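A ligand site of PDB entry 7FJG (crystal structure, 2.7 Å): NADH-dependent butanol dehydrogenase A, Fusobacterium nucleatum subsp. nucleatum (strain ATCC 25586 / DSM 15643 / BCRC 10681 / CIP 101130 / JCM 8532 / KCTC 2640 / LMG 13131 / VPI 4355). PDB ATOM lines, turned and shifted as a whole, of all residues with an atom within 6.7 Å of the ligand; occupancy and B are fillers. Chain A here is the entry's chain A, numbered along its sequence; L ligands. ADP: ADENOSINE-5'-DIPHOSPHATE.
A nitrogen (N6) of the ligand sits at hydrogen-bond distance from the backbone carbonyl oxygen (O) of Thr 143, 2.6 Å away.
A nitrogen (N7) of the ligand sits at hydrogen-bond distance from the side-chain hydroxyl (OG1) of Thr 143 (3.3 Å).
O of Val 184 lies within hydrogen-bond range of N6 of the ligand (2.8 Å).
N of Ala 103 is in hydrogen-bond range of O3B of the ligand.
The backbone NH of Thr 143 lies within hydrogen-bond range of the backbone carbonyl oxygen of Gly 101.
The side-chain hydroxyl (OG) of Ser 104 lies within hydrogen-bond range of the backbone carbonyl oxygen (O) of Pro 75, at 2.5 Å.
OE1 of Glu 41 sits close to N of Val 74 (3.2 Å).
Glu 41 touches the ligand (OE2 to O2A, 3.96 Å).
Leu 46 touches the ligand.
Leu 50 touches the ligand.
Gly 102 touches the ligand.
Ser 104 touches the ligand (OG to O2B, 3.8 Å).
Ile 144 touches the ligand.
Gly 146 touches the ligand (O to O3B, 3.6 Å).
Thr 187 touches the ligand (CG2 to N1, 3.2 Å).
CG1 of Ile 188 touches N1 of the ligand, at 3.4 Å.
Leu 192 touches the ligand (CD1 to O4', 3.8 Å).
13 residues have an atom within 4 Å of the ligand: Glu 41, Leu 46, Leu 50, Gly 102, Ala 103, Ser 104, Thr 143, Ile 144, Gly 146, Val 184, Thr 187, Ile 188 and Leu 192.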
ATOM      1  N   GLU A  41      26.148  -1.525  17.358  1.00  0.00           N
ATOM      2  CA  GLU A  41      25.894  -0.409  16.450  1.00  0.00           C
ATOM      3  C   GLU A  41      27.219   0.084  15.867  1.00  0.00           C
ATOM      4  O   GLU A  41      28.207   0.214  16.585  1.00  0.00           O
ATOM      5  CB  GLU A  41      25.191   0.751  17.165  1.00  0.00           C
ATOM      6  CG  GLU A  41      23.676   0.561  17.391  1.00  0.00           C
ATOM      7  CD  GLU A  41      22.797   1.722  16.859  1.00  0.00           C
ATOM      8  OE1 GLU A  41      22.180   1.551  15.789  1.00  0.00           O
ATOM      9  OE2 GLU A  41      22.711   2.796  17.518  1.00  0.00           O
ATOM     10  N   LEU A  46      31.369   3.039  20.455  1.00  0.00           N
ATOM     11  CA  LEU A  46      31.062   3.343  21.838  1.00  0.00           C
ATOM     12  C   LEU A  46      31.450   2.195  22.788  1.00  0.00           C
ATOM     13  O   LEU A  46      32.247   2.393  23.703  1.00  0.00           O
ATOM     14  CB  LEU A  46      29.575   3.691  21.993  1.00  0.00           C
ATOM     15  CG  LEU A  46      29.196   4.139  23.415  1.00  0.00           C
ATOM     16  CD1 LEU A  46      28.622   5.532  23.531  1.00  0.00           C
ATOM     17  CD2 LEU A  46      28.215   3.125  24.003  1.00  0.00           C
ATOM     18  N   LEU A  50      34.020   2.858  25.893  1.00  0.00           N
ATOM     19  CA  LEU A  50      33.615   2.661  27.274  1.00  0.00           C
ATOM     20  C   LEU A  50      34.359   1.511  27.950  1.00  0.00           C
ATOM     21  O   LEU A  50      34.245   1.369  29.170  1.00  0.00           O
ATOM     22  CB  LEU A  50      32.109   2.377  27.358  1.00  0.00           C
ATOM     23  CG  LEU A  50      31.161   3.283  26.557  1.00  0.00           C
ATOM     24  CD1 LEU A  50      29.683   3.081  26.860  1.00  0.00           C
ATOM     25  CD2 LEU A  50      31.531   4.739  26.808  1.00  0.00           C
ATOM     26  N   VAL A  74      21.883   0.732  12.690  1.00  0.00           N
ATOM     27  CA  VAL A  74      21.343   2.085  12.609  1.00  0.00           C
ATOM     28  C   VAL A  74      20.369   2.246  13.771  1.00  0.00           C
ATOM     29  O   VAL A  74      19.737   1.258  14.191  1.00  0.00           O
ATOM     30  CB  VAL A  74      20.678   2.355  11.249  1.00  0.00           C
ATOM     31  CG1 VAL A  74      19.549   1.409  10.971  1.00  0.00           C
ATOM     32  CG2 VAL A  74      20.117   3.767  11.137  1.00  0.00           C
ATOM     33  N   PRO A  75      20.232   3.448  14.322  1.00  0.00           N
ATOM     34  CA  PRO A  75      19.303   3.625  15.450  1.00  0.00           C
ATOM     35  C   PRO A  75      17.929   2.988  15.252  1.00  0.00           C
ATOM     36  O   PRO A  75      17.361   2.527  16.241  1.00  0.00           O
ATOM     37  CB  PRO A  75      19.218   5.147  15.604  1.00  0.00           C
ATOM     38  CG  PRO A  75      20.414   5.713  14.897  1.00  0.00           C
ATOM     39  CD  PRO A  75      21.157   4.591  14.202  1.00  0.00           C
ATOM     40  N   GLY A 101      24.723  -3.627  23.475  1.00  0.00           N
ATOM     41  CA  GLY A 101      24.315  -2.291  23.129  1.00  0.00           C
ATOM     42  C   GLY A 101      22.964  -1.875  23.658  1.00  0.00           C
ATOM     43  O   GLY A 101      22.673  -2.079  24.852  1.00  0.00           O
ATOM     44  N   GLY A 102      22.152  -1.272  22.791  1.00  0.00           N
ATOM     45  CA  GLY A 102      20.809  -0.850  23.139  1.00  0.00           C
ATOM     46  C   GLY A 102      19.744  -1.462  22.260  1.00  0.00           C
ATOM     47  O   GLY A 102      20.013  -2.366  21.454  1.00  0.00           O
ATOM     48  N   ALA A 103      18.532  -0.935  22.374  1.00  0.00           N
ATOM     49  CA  ALA A 103      17.365  -1.669  21.924  1.00  0.00           C
ATOM     50  C   ALA A 103      17.388  -1.930  20.441  1.00  0.00           C
ATOM     51  O   ALA A 103      16.782  -2.886  19.963  1.00  0.00           O
ATOM     52  CB  ALA A 103      16.100  -0.893  22.297  1.00  0.00           C
ATOM     53  N   SER A 104      18.081  -1.100  19.686  1.00  0.00           N
ATOM     54  CA  SER A 104      18.076  -1.278  18.254  1.00  0.00           C
ATOM     55  C   SER A 104      19.167  -2.210  17.742  1.00  0.00           C
ATOM     56  O   SER A 104      19.131  -2.576  16.572  1.00  0.00           O
ATOM     57  CB  SER A 104      18.174   0.092  17.600  1.00  0.00           C
ATOM     58  OG  SER A 104      17.358   1.025  18.301  1.00  0.00           O
ATOM     59  N   VAL A 105      20.158  -2.593  18.545  1.00  0.00           N
ATOM     60  CA  VAL A 105      20.934  -3.791  18.211  1.00  0.00           C
ATOM     61  C   VAL A 105      20.292  -5.013  18.843  1.00  0.00           C
ATOM     62  O   VAL A 105      20.197  -6.056  18.188  1.00  0.00           O
ATOM     63  CB  VAL A 105      22.420  -3.661  18.610  1.00  0.00           C
ATOM     64  CG1 VAL A 105      22.967  -2.292  18.246  1.00  0.00           C
ATOM     65  CG2 VAL A 105      22.618  -3.985  20.076  1.00  0.00           C
ATOM     66  N   LEU A 142      23.357  -4.953  28.120  1.00  0.00           N
ATOM     67  CA  LEU A 142      22.642  -3.699  27.896  1.00  0.00           C
ATOM     68  C   LEU A 142      23.550  -2.561  28.306  1.00  0.00           C
ATOM     69  O   LEU A 142      24.160  -2.610  29.380  1.00  0.00           O
ATOM     70  CB  LEU A 142      21.362  -3.648  28.714  1.00  0.00           C
ATOM     71  CG  LEU A 142      20.322  -2.559  28.415  1.00  0.00           C
ATOM     72  CD1 LEU A 142      19.534  -2.922  27.152  1.00  0.00           C
ATOM     73  CD2 LEU A 142      19.414  -2.335  29.640  1.00  0.00           C
ATOM     74  N   THR A 143      23.652  -1.548  27.437  1.00  0.00           N
ATOM     75  CA  THR A 143      24.409  -0.355  27.738  1.00  0.00           C
ATOM     76  C   THR A 143      23.515   0.830  28.074  1.00  0.00           C
ATOM     77  O   THR A 143      24.029   1.819  28.604  1.00  0.00           O
ATOM     78  CB  THR A 143      25.323   0.005  26.556  1.00  0.00           C
ATOM     79  OG1 THR A 143      24.523   0.264  25.397  1.00  0.00           O
ATOM     80  CG2 THR A 143      26.298  -1.140  26.269  1.00  0.00           C
ATOM     81  N   ILE A 144      22.212   0.762  27.818  1.00  0.00           N
ATOM     82  CA  ILE A 144      21.344   1.886  28.156  1.00  0.00           C
ATOM     83  C   ILE A 144      19.946   1.432  28.568  1.00  0.00           C
ATOM     84  O   ILE A 144      19.195   0.908  27.724  1.00  0.00           O
ATOM     85  CB  ILE A 144      21.289   2.884  26.986  1.00  0.00           C
ATOM     86  CG1 ILE A 144      20.585   4.158  27.435  1.00  0.00           C
ATOM     87  CG2 ILE A 144      20.607   2.265  25.783  1.00  0.00           C
ATOM     88  CD1 ILE A 144      20.698   5.319  26.456  1.00  0.00           C
ATOM     89  N   PRO A 145      19.520   1.665  29.859  1.00  0.00           N
ATOM     90  CA  PRO A 145      18.229   1.090  30.362  1.00  0.00           C
ATOM     91  C   PRO A 145      16.985   1.827  29.872  1.00  0.00           C
ATOM     92  O   PRO A 145      16.206   2.462  30.623  1.00  0.00           O
ATOM     93  CB  PRO A 145      18.416   1.152  31.876  1.00  0.00           C
ATOM     94  CG  PRO A 145      19.306   2.357  32.103  1.00  0.00           C
ATOM     95  CD  PRO A 145      20.234   2.437  30.892  1.00  0.00           C
ATOM     96  N   GLY A 146      16.738   1.709  28.579  1.00  0.00           N
ATOM     97  CA  GLY A 146      15.557   2.281  27.958  1.00  0.00           C
ATOM     98  C   GLY A 146      14.775   1.233  27.214  1.00  0.00           C
ATOM     99  O   GLY A 146      15.356   0.374  26.541  1.00  0.00           O
ATOM    100  N   ALA A 147      13.451   1.268  27.374  1.00  0.00           N
ATOM    101  CA  ALA A 147      12.496   0.492  26.591  1.00  0.00           C
ATOM    102  C   ALA A 147      12.455  -1.007  26.923  1.00  0.00           C
ATOM    103  O   ALA A 147      11.445  -1.647  26.647  1.00  0.00           O
ATOM    104  CB  ALA A 147      12.773   0.634  25.096  1.00  0.00           C
ATOM    105  N   GLY A 148      13.514  -1.578  27.495  1.00  0.00           N
ATOM    106  CA  GLY A 148      13.456  -2.946  27.970  1.00  0.00           C
ATOM    107  C   GLY A 148      13.432  -4.041  26.922  1.00  0.00           C
ATOM    108  O   GLY A 148      13.055  -5.169  27.240  1.00  0.00           O
ATOM    109  N   GLU A 183      26.616   0.450  36.137  1.00  0.00           N
ATOM    110  CA  GLU A 183      27.779   1.270  35.822  1.00  0.00           C
ATOM    111  C   GLU A 183      27.653   1.884  34.438  1.00  0.00           C
ATOM    112  O   GLU A 183      28.114   3.001  34.215  1.00  0.00           O
ATOM    113  CB  GLU A 183      29.075   0.447  35.903  1.00  0.00           C
ATOM    114  CG  GLU A 183      29.586   0.047  37.326  1.00  0.00           C
ATOM    115  CD  GLU A 183      30.927  -0.724  37.316  1.00  0.00           C
ATOM    116  OE1 GLU A 183      30.971  -1.878  36.800  1.00  0.00           O
ATOM    117  OE2 GLU A 183      31.951  -0.185  37.815  1.00  0.00           O
ATOM    118  N   VAL A 184      27.001   1.190  33.499  1.00  0.00           N
ATOM    119  CA  VAL A 184      26.850   1.722  32.140  1.00  0.00           C
ATOM    120  C   VAL A 184      26.045   3.016  32.090  1.00  0.00           C
ATOM    121  O   VAL A 184      26.025   3.689  31.050  1.00  0.00           O
ATOM    122  CB  VAL A 184      26.192   0.709  31.179  1.00  0.00           C
ATOM    123  CG1 VAL A 184      26.866  -0.619  31.314  1.00  0.00           C
ATOM    124  CG2 VAL A 184      24.647   0.594  31.416  1.00  0.00           C
ATOM    125  N   CYS A 185      25.322   3.331  33.167  1.00  0.00           N
ATOM    126  CA  CYS A 185      24.550   4.578  33.234  1.00  0.00           C
ATOM    127  C   CYS A 185      25.483   5.798  33.283  1.00  0.00           C
ATOM    128  O   CYS A 185      25.135   6.869  32.746  1.00  0.00           O
ATOM    129  CB  CYS A 185      23.622   4.484  34.463  1.00  0.00           C
ATOM    130  SG  CYS A 185      21.946   3.708  34.135  1.00  0.00           S
ATOM    131  N   TYR A 186      26.711   5.619  33.806  1.00  0.00           N
ATOM    132  CA  TYR A 186      27.548   6.753  34.178  1.00  0.00           C
ATOM    133  C   TYR A 186      27.877   7.636  32.990  1.00  0.00           C
ATOM    134  O   TYR A 186      27.791   8.867  33.058  1.00  0.00           O
ATOM    135  CB  TYR A 186      28.853   6.271  34.804  1.00  0.00           C
ATOM    136  CG  TYR A 186      28.756   5.479  36.071  1.00  0.00           C
ATOM    137  CD1 TYR A 186      27.532   5.287  36.687  1.00  0.00           C
ATOM    138  CD2 TYR A 186      29.889   4.920  36.658  1.00  0.00           C
ATOM    139  CE1 TYR A 186      27.440   4.565  37.856  1.00  0.00           C
ATOM    140  CE2 TYR A 186      29.804   4.183  37.831  1.00  0.00           C
ATOM    141  CZ  TYR A 186      28.580   4.020  38.413  1.00  0.00           C
ATOM    142  OH  TYR A 186      28.478   3.285  39.577  1.00  0.00           O
ATOM    143  N   THR A 187      28.342   7.034  31.898  1.00  0.00           N
ATOM    144  CA  THR A 187      28.803   7.801  30.757  1.00  0.00           C
ATOM    145  C   THR A 187      27.664   8.432  29.968  1.00  0.00           C
ATOM    146  O   THR A 187      27.922   9.183  29.025  1.00  0.00           O
ATOM    147  CB  THR A 187      29.673   6.898  29.881  1.00  0.00           C
ATOM    148  OG1 THR A 187      29.893   7.525  28.603  1.00  0.00           O
ATOM    149  CG2 THR A 187      29.037   5.496  29.667  1.00  0.00           C
ATOM    150  N   ILE A 188      26.409   8.194  30.338  1.00  0.00           N
ATOM    151  CA  ILE A 188      25.287   8.659  29.498  1.00  0.00           C
ATOM    152  C   ILE A 188      25.140  10.175  29.619  1.00  0.00           C
ATOM    153  O   ILE A 188      25.192  10.711  30.737  1.00  0.00           O
ATOM    154  CB  ILE A 188      23.995   7.941  29.929  1.00  0.00           C
ATOM    155  CG1 ILE A 188      24.136   6.426  29.693  1.00  0.00           C
ATOM    156  CG2 ILE A 188      22.763   8.499  29.209  1.00  0.00           C
ATOM    157  CD1 ILE A 188      22.851   5.636  29.779  1.00  0.00           C
ATOM    158  N   PRO A 189      24.932  10.900  28.537  1.00  0.00           N
ATOM    159  CA  PRO A 189      24.814  12.370  28.677  1.00  0.00           C
ATOM    160  C   PRO A 189      23.539  12.805  29.407  1.00  0.00           C
ATOM    161  O   PRO A 189      22.505  12.111  29.413  1.00  0.00           O
ATOM    162  CB  PRO A 189      24.818  12.896  27.225  1.00  0.00           C
ATOM    163  CG  PRO A 189      25.122  11.701  26.330  1.00  0.00           C
ATOM    164  CD  PRO A 189      24.795  10.453  27.134  1.00  0.00           C
ATOM    165  N   LEU A 192      20.073  13.000  27.819  1.00  0.00           N
ATOM    166  CA  LEU A 192      19.635  11.652  27.508  1.00  0.00           C
ATOM    167  C   LEU A 192      19.377  10.837  28.770  1.00  0.00           C
ATOM    168  O   LEU A 192      18.553   9.931  28.743  1.00  0.00           O
ATOM    169  CB  LEU A 192      20.667  10.970  26.640  1.00  0.00           C
ATOM    170  CG  LEU A 192      20.201   9.846  25.742  1.00  0.00           C
ATOM    171  CD1 LEU A 192      20.958   9.997  24.441  1.00  0.00           C
ATOM    172  CD2 LEU A 192      20.470   8.514  26.383  1.00  0.00           C
HETATM  173  PB  ADP L   1      17.792   2.846  22.974  1.00  0.00           P
HETATM  174  O1B ADP L   1      17.782   4.266  23.554  1.00  0.00           O
HETATM  175  O2B ADP L   1      17.063   2.661  21.667  1.00  0.00           O
HETATM  176  O3B ADP L   1      17.467   1.791  24.031  1.00  0.00           O
HETATM  177  PA  ADP L   1      20.357   3.621  21.704  1.00  0.00           P
HETATM  178  O1A ADP L   1      21.742   3.172  22.130  1.00  0.00           O
HETATM  179  O2A ADP L   1      20.000   3.773  20.237  1.00  0.00           O
HETATM  180  O3A ADP L   1      19.284   2.583  22.349  1.00  0.00           O
HETATM  181  O5' ADP L   1      20.319   5.059  22.444  1.00  0.00           O
HETATM  182  C5' ADP L   1      20.524   6.259  21.682  1.00  0.00           C
HETATM  183  C4' ADP L   1      21.892   6.888  21.951  1.00  0.00           C
HETATM  184  O4' ADP L   1      22.334   6.626  23.279  1.00  0.00           O
HETATM  185  C3' ADP L   1      22.974   6.328  21.020  1.00  0.00           C
HETATM  186  O3' ADP L   1      23.436   7.366  20.150  1.00  0.00           O
HETATM  187  C2' ADP L   1      24.153   5.970  21.883  1.00  0.00           C
HETATM  188  O2' ADP L   1      25.227   6.837  21.509  1.00  0.00           O
HETATM  189  C1' ADP L   1      23.756   6.350  23.301  1.00  0.00           C
HETATM  190  N9  ADP L   1      24.105   5.365  24.380  1.00  0.00           N
HETATM  191  C8  ADP L   1      23.608   4.124  24.577  1.00  0.00           C
HETATM  192  N7  ADP L   1      24.149   3.535  25.691  1.00  0.00           N
HETATM  193  C5  ADP L   1      25.006   4.409  26.238  1.00  0.00           C
HETATM  194  C6  ADP L   1      25.895   4.473  27.414  1.00  0.00           C
HETATM  195  N6  ADP L   1      26.029   3.451  28.291  1.00  0.00           N
HETATM  196  N1  ADP L   1      26.620   5.585  27.607  1.00  0.00           N
HETATM  197  C2  ADP L   1      26.549   6.635  26.770  1.00  0.00           C
HETATM  198  N3  ADP L   1      25.750   6.637  25.695  1.00  0.00           N
HETATM  199  C4  ADP L   1      24.977   5.588  25.375  1.00  0.00           C
